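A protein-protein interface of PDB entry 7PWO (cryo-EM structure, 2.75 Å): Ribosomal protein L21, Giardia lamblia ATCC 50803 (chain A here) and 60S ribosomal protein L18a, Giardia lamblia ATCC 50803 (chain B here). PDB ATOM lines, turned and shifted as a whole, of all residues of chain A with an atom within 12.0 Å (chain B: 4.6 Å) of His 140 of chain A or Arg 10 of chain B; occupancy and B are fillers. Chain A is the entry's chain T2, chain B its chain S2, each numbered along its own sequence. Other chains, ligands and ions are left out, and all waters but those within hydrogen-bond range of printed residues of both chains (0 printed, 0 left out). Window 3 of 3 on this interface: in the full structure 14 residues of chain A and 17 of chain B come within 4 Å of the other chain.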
ATOM      1  N   LEU A 135     -42.267 -11.122   2.047  1.00  0.00           N
ATOM      2  CA  LEU A 135     -41.323 -10.030   2.155  1.00  0.00           C
ATOM      3  C   LEU A 135     -39.973 -10.531   2.651  1.00  0.00           C
ATOM      4  O   LEU A 135     -39.858 -11.653   3.150  1.00  0.00           O
ATOM      5  CB  LEU A 135     -41.872  -8.971   3.103  1.00  0.00           C
ATOM      6  CG  LEU A 135     -43.174  -8.301   2.661  1.00  0.00           C
ATOM      7  CD1 LEU A 135     -44.049  -7.956   3.849  1.00  0.00           C
ATOM      8  CD2 LEU A 135     -42.863  -7.069   1.844  1.00  0.00           C
ATOM      9  N   PRO A 136     -38.922  -9.727   2.495  1.00  0.00           N
ATOM     10  CA  PRO A 136     -37.687 -10.002   3.232  1.00  0.00           C
ATOM     11  C   PRO A 136     -37.931  -9.939   4.732  1.00  0.00           C
ATOM     12  O   PRO A 136     -38.734  -9.142   5.221  1.00  0.00           O
ATOM     13  CB  PRO A 136     -36.731  -8.901   2.760  1.00  0.00           C
ATOM     14  CG  PRO A 136     -37.587  -7.890   2.095  1.00  0.00           C
ATOM     15  CD  PRO A 136     -38.760  -8.611   1.551  1.00  0.00           C
ATOM     16  N   ARG A 137     -37.226 -10.795   5.459  1.00  0.00           N
ATOM     17  CA  ARG A 137     -37.455 -10.995   6.881  1.00  0.00           C
ATOM     18  C   ARG A 137     -36.810  -9.872   7.690  1.00  0.00           C
ATOM     19  O   ARG A 137     -35.809  -9.283   7.282  1.00  0.00           O
ATOM     20  CB  ARG A 137     -36.898 -12.362   7.270  1.00  0.00           C
ATOM     21  CG  ARG A 137     -35.411 -12.400   7.172  1.00  0.00           C
ATOM     22  CD  ARG A 137     -34.807 -13.755   7.408  1.00  0.00           C
ATOM     23  NE  ARG A 137     -35.162 -14.629   6.297  1.00  0.00           N
ATOM     24  CZ  ARG A 137     -34.914 -15.933   6.246  1.00  0.00           C
ATOM     25  NH1 ARG A 137     -34.282 -16.527   7.240  1.00  0.00           N
ATOM     26  NH2 ARG A 137     -35.264 -16.631   5.178  1.00  0.00           N
ATOM     27  N   ALA A 138     -37.390  -9.588   8.854  1.00  0.00           N
ATOM     28  CA  ALA A 138     -37.008  -8.444   9.667  1.00  0.00           C
ATOM     29  C   ALA A 138     -35.798  -8.752  10.548  1.00  0.00           C
ATOM     30  O   ALA A 138     -35.374  -9.902  10.701  1.00  0.00           O
ATOM     31  CB  ALA A 138     -38.175  -7.995  10.542  1.00  0.00           C
ATOM     32  N   ALA A 139     -35.258  -7.691  11.149  1.00  0.00           N
ATOM     33  CA  ALA A 139     -34.132  -7.804  12.066  1.00  0.00           C
ATOM     34  C   ALA A 139     -34.557  -8.436  13.389  1.00  0.00           C
ATOM     35  O   ALA A 139     -35.666  -8.207  13.875  1.00  0.00           O
ATOM     36  CB  ALA A 139     -33.527  -6.432  12.321  1.00  0.00           C
ATOM     37  N   HIS A 140     -33.660  -9.227  13.980  1.00  0.00           N
ATOM     38  CA  HIS A 140     -33.983  -9.962  15.198  1.00  0.00           C
ATOM     39  C   HIS A 140     -32.692 -10.391  15.887  1.00  0.00           C
ATOM     40  O   HIS A 140     -31.587 -10.096  15.431  1.00  0.00           O
ATOM     41  CB  HIS A 140     -34.854 -11.184  14.893  1.00  0.00           C
ATOM     42  CG  HIS A 140     -34.296 -12.062  13.822  1.00  0.00           C
ATOM     43  ND1 HIS A 140     -34.485 -11.809  12.484  1.00  0.00           N
ATOM     44  CD2 HIS A 140     -33.576 -13.204  13.892  1.00  0.00           C
ATOM     45  CE1 HIS A 140     -33.891 -12.749  11.772  1.00  0.00           C
ATOM     46  NE2 HIS A 140     -33.331 -13.608  12.603  1.00  0.00           N
ATOM     47  N   VAL A 141     -32.852 -11.118  16.993  1.00  0.00           N
ATOM     48  CA  VAL A 141     -31.752 -11.556  17.845  1.00  0.00           C
ATOM     49  C   VAL A 141     -31.738 -13.073  17.921  1.00  0.00           C
ATOM     50  O   VAL A 141     -32.782 -13.707  18.110  1.00  0.00           O
ATOM     51  CB  VAL A 141     -31.852 -10.954  19.256  1.00  0.00           C
ATOM     52  CG1 VAL A 141     -30.768 -11.526  20.133  1.00  0.00           C
ATOM     53  CG2 VAL A 141     -31.704  -9.439  19.182  1.00  0.00           C
ATOM     54  N   VAL A 142     -30.553 -13.652  17.780  1.00  0.00           N
ATOM     55  CA  VAL A 142     -30.337 -15.069  18.024  1.00  0.00           C
ATOM     56  C   VAL A 142     -29.194 -15.207  19.017  1.00  0.00           C
ATOM     57  O   VAL A 142     -28.171 -14.530  18.889  1.00  0.00           O
ATOM     58  CB  VAL A 142     -30.029 -15.836  16.727  1.00  0.00           C
ATOM     59  CG1 VAL A 142     -29.881 -17.300  17.012  1.00  0.00           C
ATOM     60  CG2 VAL A 142     -31.138 -15.620  15.730  1.00  0.00           C
ATOM     61  N   SER A 143     -29.384 -16.058  20.020  1.00  0.00           N
ATOM     62  CA  SER A 143     -28.295 -16.417  20.910  1.00  0.00           C
ATOM     63  C   SER A 143     -27.326 -17.361  20.212  1.00  0.00           C
ATOM     64  O   SER A 143     -27.710 -18.167  19.363  1.00  0.00           O
ATOM     65  CB  SER A 143     -28.838 -17.069  22.175  1.00  0.00           C
ATOM     66  OG  SER A 143     -29.004 -18.462  21.989  1.00  0.00           O
ATOM     67  N   ILE A 144     -26.050 -17.239  20.569  1.00  0.00           N
ATOM     68  CA  ILE A 144     -24.991 -18.101  20.052  1.00  0.00           C
ATOM     69  C   ILE A 144     -24.164 -18.675  21.190  1.00  0.00           C
ATOM     70  O   ILE A 144     -22.984 -18.999  21.018  1.00  0.00           O
ATOM     71  CB  ILE A 144     -24.108 -17.345  19.048  1.00  0.00           C
ATOM     72  CG1 ILE A 144     -23.426 -16.154  19.737  1.00  0.00           C
ATOM     73  CG2 ILE A 144     -24.914 -16.955  17.829  1.00  0.00           C
ATOM     74  CD1 ILE A 144     -22.378 -15.479  18.919  1.00  0.00           C
ATOM     75  N   ALA A 145     -24.785 -18.841  22.352  1.00  0.00           N
ATOM     76  CA  ALA A 145     -24.069 -19.364  23.504  1.00  0.00           C
ATOM     77  C   ALA A 145     -23.655 -20.827  23.344  1.00  0.00           C
ATOM     78  O   ALA A 145     -22.818 -21.298  24.120  1.00  0.00           O
ATOM     79  CB  ALA A 145     -24.921 -19.195  24.762  1.00  0.00           C
ATOM     80  N   SER A 146     -24.196 -21.551  22.365  1.00  0.00           N
ATOM     81  CA  SER A 146     -23.960 -22.990  22.230  1.00  0.00           C
ATOM     82  C   SER A 146     -23.653 -23.387  20.786  1.00  0.00           C
ATOM     83  O   SER A 146     -24.248 -24.313  20.232  1.00  0.00           O
ATOM     84  CB  SER A 146     -25.149 -23.776  22.766  1.00  0.00           C
ATOM     85  OG  SER A 146     -24.970 -25.161  22.556  1.00  0.00           O
ATOM     86  N   ALA A 147     -22.716 -22.695  20.152  1.00  0.00           N
ATOM     87  CA  ALA A 147     -22.372 -22.985  18.768  1.00  0.00           C
ATOM     88  C   ALA A 147     -21.745 -24.370  18.612  1.00  0.00           C
ATOM     89  O   ALA A 147     -21.059 -24.877  19.506  1.00  0.00           O
ATOM     90  CB  ALA A 147     -21.418 -21.926  18.235  1.00  0.00           C
ATOM     91  N   ILE A 148     -21.999 -24.980  17.456  1.00  0.00           N
ATOM     92  CA  ILE A 148     -21.379 -26.234  17.032  1.00  0.00           C
ATOM     93  C   ILE A 148     -20.440 -25.914  15.881  1.00  0.00           C
ATOM     94  O   ILE A 148     -20.837 -25.241  14.925  1.00  0.00           O
ATOM     95  CB  ILE A 148     -22.430 -27.268  16.590  1.00  0.00           C
ATOM     96  CG1 ILE A 148     -23.654 -27.213  17.498  1.00  0.00           C
ATOM     97  CG2 ILE A 148     -21.837 -28.674  16.527  1.00  0.00           C
ATOM     98  CD1 ILE A 148     -24.803 -28.045  17.003  1.00  0.00           C
ATOM     99  N   ASP A 149     -19.199 -26.377  15.971  1.00  0.00           N
ATOM    100  CA  ASP A 149     -18.176 -26.045  14.987  1.00  0.00           C
ATOM    101  C   ASP A 149     -17.912 -27.248  14.108  1.00  0.00           C
ATOM    102  O   ASP A 149     -17.489 -28.299  14.600  1.00  0.00           O
ATOM    103  CB  ASP A 149     -16.887 -25.577  15.660  1.00  0.00           C
ATOM    104  CG  ASP A 149     -17.004 -24.172  16.201  1.00  0.00           C
ATOM    105  OD1 ASP A 149     -18.118 -23.809  16.627  1.00  0.00           O
ATOM    106  OD2 ASP A 149     -15.998 -23.432  16.183  1.00  0.00           O
ATOM    107  N   ILE A 150     -18.133 -27.083  12.807  1.00  0.00           N
ATOM    108  CA  ILE A 150     -17.963 -28.164  11.852  1.00  0.00           C
ATOM    109  C   ILE A 150     -16.962 -27.746  10.786  1.00  0.00           C
ATOM    110  O   ILE A 150     -16.646 -26.569  10.614  1.00  0.00           O
ATOM    111  CB  ILE A 150     -19.297 -28.591  11.216  1.00  0.00           C
ATOM    112  CG1 ILE A 150     -19.920 -27.445  10.431  1.00  0.00           C
ATOM    113  CG2 ILE A 150     -20.250 -29.089  12.283  1.00  0.00           C
ATOM    114  CD1 ILE A 150     -21.101 -27.881   9.605  1.00  0.00           C
ATOM    115  N   GLY B   9     -24.374 -19.473  10.871  1.00  0.00           N
ATOM    116  CA  GLY B   9     -25.598 -19.734  10.135  1.00  0.00           C
ATOM    117  C   GLY B   9     -26.461 -20.764  10.835  1.00  0.00           C
ATOM    118  O   GLY B   9     -26.031 -21.412  11.793  1.00  0.00           O
ATOM    119  N   ARG B  10     -27.701 -20.907  10.352  1.00  0.00           N
ATOM    120  CA  ARG B  10     -28.645 -21.823  10.996  1.00  0.00           C
ATOM    121  C   ARG B  10     -29.800 -22.164  10.063  1.00  0.00           C
ATOM    122  O   ARG B  10     -30.022 -21.499   9.052  1.00  0.00           O
ATOM    123  CB  ARG B  10     -29.197 -21.236  12.302  1.00  0.00           C
ATOM    124  CG  ARG B  10     -30.028 -19.980  12.124  1.00  0.00           C
ATOM    125  CD  ARG B  10     -31.036 -19.831  13.238  1.00  0.00           C
ATOM    126  NE  ARG B  10     -31.873 -18.651  13.060  1.00  0.00           N
ATOM    127  CZ  ARG B  10     -32.699 -18.166  13.979  1.00  0.00           C
ATOM    128  NH1 ARG B  10     -33.419 -17.089  13.712  1.00  0.00           N
ATOM    129  NH2 ARG B  10     -32.808 -18.754  15.161  1.00  0.00           N
ATOM    130  N   ARG B  11     -30.519 -23.233  10.411  1.00  0.00           N
ATOM    131  CA  ARG B  11     -31.780 -23.571   9.758  1.00  0.00           C
ATOM    132  C   ARG B  11     -32.862 -22.585  10.178  1.00  0.00           C
ATOM    133  O   ARG B  11     -32.867 -22.082  11.303  1.00  0.00           O
ATOM    134  CB  ARG B  11     -32.226 -24.984  10.133  1.00  0.00           C
ATOM    135  CG  ARG B  11     -33.545 -25.415   9.514  1.00  0.00           C
ATOM    136  CD  ARG B  11     -33.918 -26.841   9.864  1.00  0.00           C
ATOM    137  NE  ARG B  11     -33.389 -27.849   8.950  1.00  0.00           N
ATOM    138  CZ  ARG B  11     -32.583 -28.838   9.327  1.00  0.00           C
ATOM    139  NH1 ARG B  11     -32.152 -29.728   8.444  1.00  0.00           N
ATOM    140  NH2 ARG B  11     -32.212 -28.942  10.594  1.00  0.00           N
ATOM    141  N   LEU B  12     -33.798 -22.317   9.275  1.00  0.00           N
ATOM    142  CA  LEU B  12     -34.832 -21.349   9.596  1.00  0.00           C
ATOM    143  C   LEU B  12     -35.866 -22.000  10.518  1.00  0.00           C
ATOM    144  O   LEU B  12     -36.284 -23.133  10.264  1.00  0.00           O
ATOM    145  CB  LEU B  12     -35.456 -20.814   8.309  1.00  0.00           C
ATOM    146  CG  LEU B  12     -36.524 -19.726   8.333  1.00  0.00           C
ATOM    147  CD1 LEU B  12     -35.942 -18.484   8.927  1.00  0.00           C
ATOM    148  CD2 LEU B  12     -36.977 -19.426   6.919  1.00  0.00           C
ATOM    149  N   PRO B  13     -36.266 -21.335  11.604  1.00  0.00           N
ATOM    150  CA  PRO B  13     -37.017 -22.022  12.664  1.00  0.00           C
ATOM    151  C   PRO B  13     -38.445 -22.383  12.285  1.00  0.00           C
ATOM    152  O   PRO B  13     -39.141 -21.635  11.595  1.00  0.00           O
ATOM    153  CB  PRO B  13     -37.004 -21.012  13.814  1.00  0.00           C
ATOM    154  CG  PRO B  13     -36.747 -19.703  13.174  1.00  0.00           C
ATOM    155  CD  PRO B  13     -35.891 -19.969  11.994  1.00  0.00           C
ATOM    156  N   PRO B  20     -33.543 -23.574  16.500  1.00  0.00           N
ATOM    157  CA  PRO B  20     -32.614 -24.546  15.909  1.00  0.00           C
ATOM    158  C   PRO B  20     -31.171 -24.247  16.297  1.00  0.00           C
ATOM    159  O   PRO B  20     -30.832 -23.176  16.798  1.00  0.00           O
ATOM    160  CB  PRO B  20     -32.814 -24.364  14.401  1.00  0.00           C
ATOM    161  CG  PRO B  20     -34.071 -23.603  14.251  1.00  0.00           C
ATOM    162  CD  PRO B  20     -34.195 -22.753  15.468  1.00  0.00           C
ATOM    163  N   GLU B  21     -30.295 -25.208  16.011  1.00  0.00           N
ATOM    164  CA  GLU B  21     -28.898 -25.084  16.399  1.00  0.00           C
ATOM    165  C   GLU B  21     -28.184 -24.019  15.558  1.00  0.00           C
ATOM    166  O   GLU B  21     -28.724 -23.469  14.598  1.00  0.00           O
ATOM    167  CB  GLU B  21     -28.188 -26.430  16.278  1.00  0.00           C
ATOM    168  N   VAL B  22     -26.954 -23.715  15.949  1.00  0.00           N
ATOM    169  CA  VAL B  22     -26.145 -22.697  15.293  1.00  0.00           C
ATOM    170  C   VAL B  22     -24.837 -23.342  14.861  1.00  0.00           C
ATOM    171  O   VAL B  22     -24.286 -24.180  15.580  1.00  0.00           O
ATOM    172  CB  VAL B  22     -25.897 -21.495  16.227  1.00  0.00           C
ATOM    173  CG1 VAL B  22     -24.998 -20.476  15.576  1.00  0.00           C
ATOM    174  CG2 VAL B  22     -27.215 -20.862  16.618  1.00  0.00           C
ATOM    175  N   TRP B  40     -22.435 -22.043   2.491  1.00  0.00           N
ATOM    176  CA  TRP B  40     -23.654 -22.760   2.134  1.00  0.00           C
ATOM    177  C   TRP B  40     -23.337 -24.088   1.463  1.00  0.00           C
ATOM    178  O   TRP B  40     -24.015 -25.085   1.717  1.00  0.00           O
ATOM    179  CB  TRP B  40     -24.551 -21.893   1.256  1.00  0.00           C
ATOM    180  CG  TRP B  40     -25.413 -20.953   2.040  1.00  0.00           C
ATOM    181  CD1 TRP B  40     -25.579 -19.627   1.814  1.00  0.00           C
ATOM    182  CD2 TRP B  40     -26.234 -21.270   3.172  1.00  0.00           C
ATOM    183  NE1 TRP B  40     -26.442 -19.095   2.724  1.00  0.00           N
ATOM    184  CE2 TRP B  40     -26.855 -20.079   3.577  1.00  0.00           C
ATOM    185  CE3 TRP B  40     -26.502 -22.442   3.884  1.00  0.00           C
ATOM    186  CZ2 TRP B  40     -27.731 -20.022   4.654  1.00  0.00           C
ATOM    187  CZ3 TRP B  40     -27.364 -22.382   4.951  1.00  0.00           C
ATOM    188  CH2 TRP B  40     -27.972 -21.185   5.325  1.00  0.00           C
ATOM    189  N   GLY B  54     -32.449 -21.868   5.234  1.00  0.00           N
ATOM    190  CA  GLY B  54     -31.721 -21.362   6.372  1.00  0.00           C
ATOM    191  C   GLY B  54     -31.303 -19.928   6.163  1.00  0.00           C
ATOM    192  O   GLY B  54     -31.578 -19.320   5.130  1.00  0.00           O
ATOM    193  N   GLU B  55     -30.635 -19.388   7.172  1.00  0.00           N
ATOM    194  CA  GLU B  55     -30.188 -18.006   7.134  1.00  0.00           C
ATOM    195  C   GLU B  55     -28.796 -17.887   7.726  1.00  0.00           C
ATOM    196  O   GLU B  55     -28.463 -18.551   8.712  1.00  0.00           O
ATOM    197  CB  GLU B  55     -31.152 -17.076   7.875  1.00  0.00           C
ATOM    198  CG  GLU B  55     -31.264 -17.325   9.358  1.00  0.00           C
ATOM    199  CD  GLU B  55     -32.256 -16.407  10.022  1.00  0.00           C
ATOM    200  OE1 GLU B  55     -32.025 -16.019  11.182  1.00  0.00           O
ATOM    201  OE2 GLU B  55     -33.273 -16.071   9.389  1.00  0.00           O
ATOM    202  N   LEU B  57     -26.409 -15.823   9.867  1.00  0.00           N
ATOM    203  CA  LEU B  57     -26.451 -14.920  10.998  1.00  0.00           C
ATOM    204  C   LEU B  57     -25.336 -13.883  10.946  1.00  0.00           C
ATOM    205  O   LEU B  57     -25.603 -12.710  11.215  1.00  0.00           O
ATOM    206  CB  LEU B  57     -26.381 -15.726  12.295  1.00  0.00           C
ATOM    207  CG  LEU B  57     -27.478 -16.783  12.491  1.00  0.00           C
ATOM    208  CD1 LEU B  57     -27.597 -17.182  13.931  1.00  0.00           C
ATOM    209  CD2 LEU B  57     -28.820 -16.263  12.006  1.00  0.00           C
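The backbone carbonyl oxygen (O) of Val 22 of chain B sits at hydrogen-bond distance from the backbone NH (N) of Ile 148 of chain A, at 3.1 Å. NH1 of Arg 137 of chain A lies within salt-bridge range of OE2 of Glu 55 of chain B, 2.4 Å away. OE1 of Glu 55 of chain B is in hydrogen-bond range of NE2 of His 140 of chain A, 3.1 Å away.
Of the 16 printed residues of chain A, 6 touch a printed residue of chain B. Printed residues of chain A that touch a printed residue of chain B: Arg 137, His 140, Val 142, Ser 143, Ala 147 and Ile 148. Among the printed residues, Asp or Glu carboxylates within 4 Å of a Lys or Arg side-chain nitrogen of the other chain: Arg 137 of chain A with Glu 55 of chain B.
Among the printed residues, pairs that only touch across the chains: Arg 137 of chain A with Leu 12 of chain B (3.1 Å), His 140 of chain A with Arg 10 of chain B (3.7 Å), Val 142 of chain A with Arg 10 of chain B (3.4 Å), Val 142 of chain A with Leu 57 of chain B (3.8 Å), Ser 143 of chain A with Val 22 of chain B (3.9 Å), Ala 147 of chain A with Val 22 of chain B (3.9 Å) and Ile 148 of chain A with Glu 21 of chain B (3.8 Å).
His 140 of chain A touches two residues of chain B. No residue of chain A comes within 4 Å of Gly 9 of chain B. Printed residues of chain A within 4 Å of Leu 12 of chain B: Arg 137. Pro 13 of chain B touches none of the printed residues of chain A. No residue of chain A comes within 4 Å of Pro 20 of chain B. Printed residues of chain A within 4 Å of Glu 21 of chain B: Ile 148. Of chain A, only Arg 137 (2.4 Å) and His 140 (3.1 Å) come within 4 Å of Glu 55 of chain B. Of the printed residues of chain B, Ile 148 of chain A touches Glu 21 and Val 22. Of the printed residues of chain B, Ala 147 of chain A touches Val 22 (3.9 Å). Trp 40 of chain B touches none of the printed residues of chain A. Ala 145 of chain A touches none of the printed residues of chain B. The nearest printed residue of chain B that does not touch His 140 of chain A is Leu 57 of chain B (5.3 Å). The nearest residue of chain A that does not touch Arg 10 of chain B is Val 141 of chain A (5.6 Å). The nearest printed residue of chain B that does not touch Arg 137 of chain A is Gly 54 of chain B (4.4 Å).
NH1 of Arg 10 of chain B lies within salt-bridge range of OE1 of Glu 55 of chain B (3.1 Å). O of Ala 138 of chain A is in hydrogen-bond range of ND1 of His 140 of chain A (2.8 Å).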
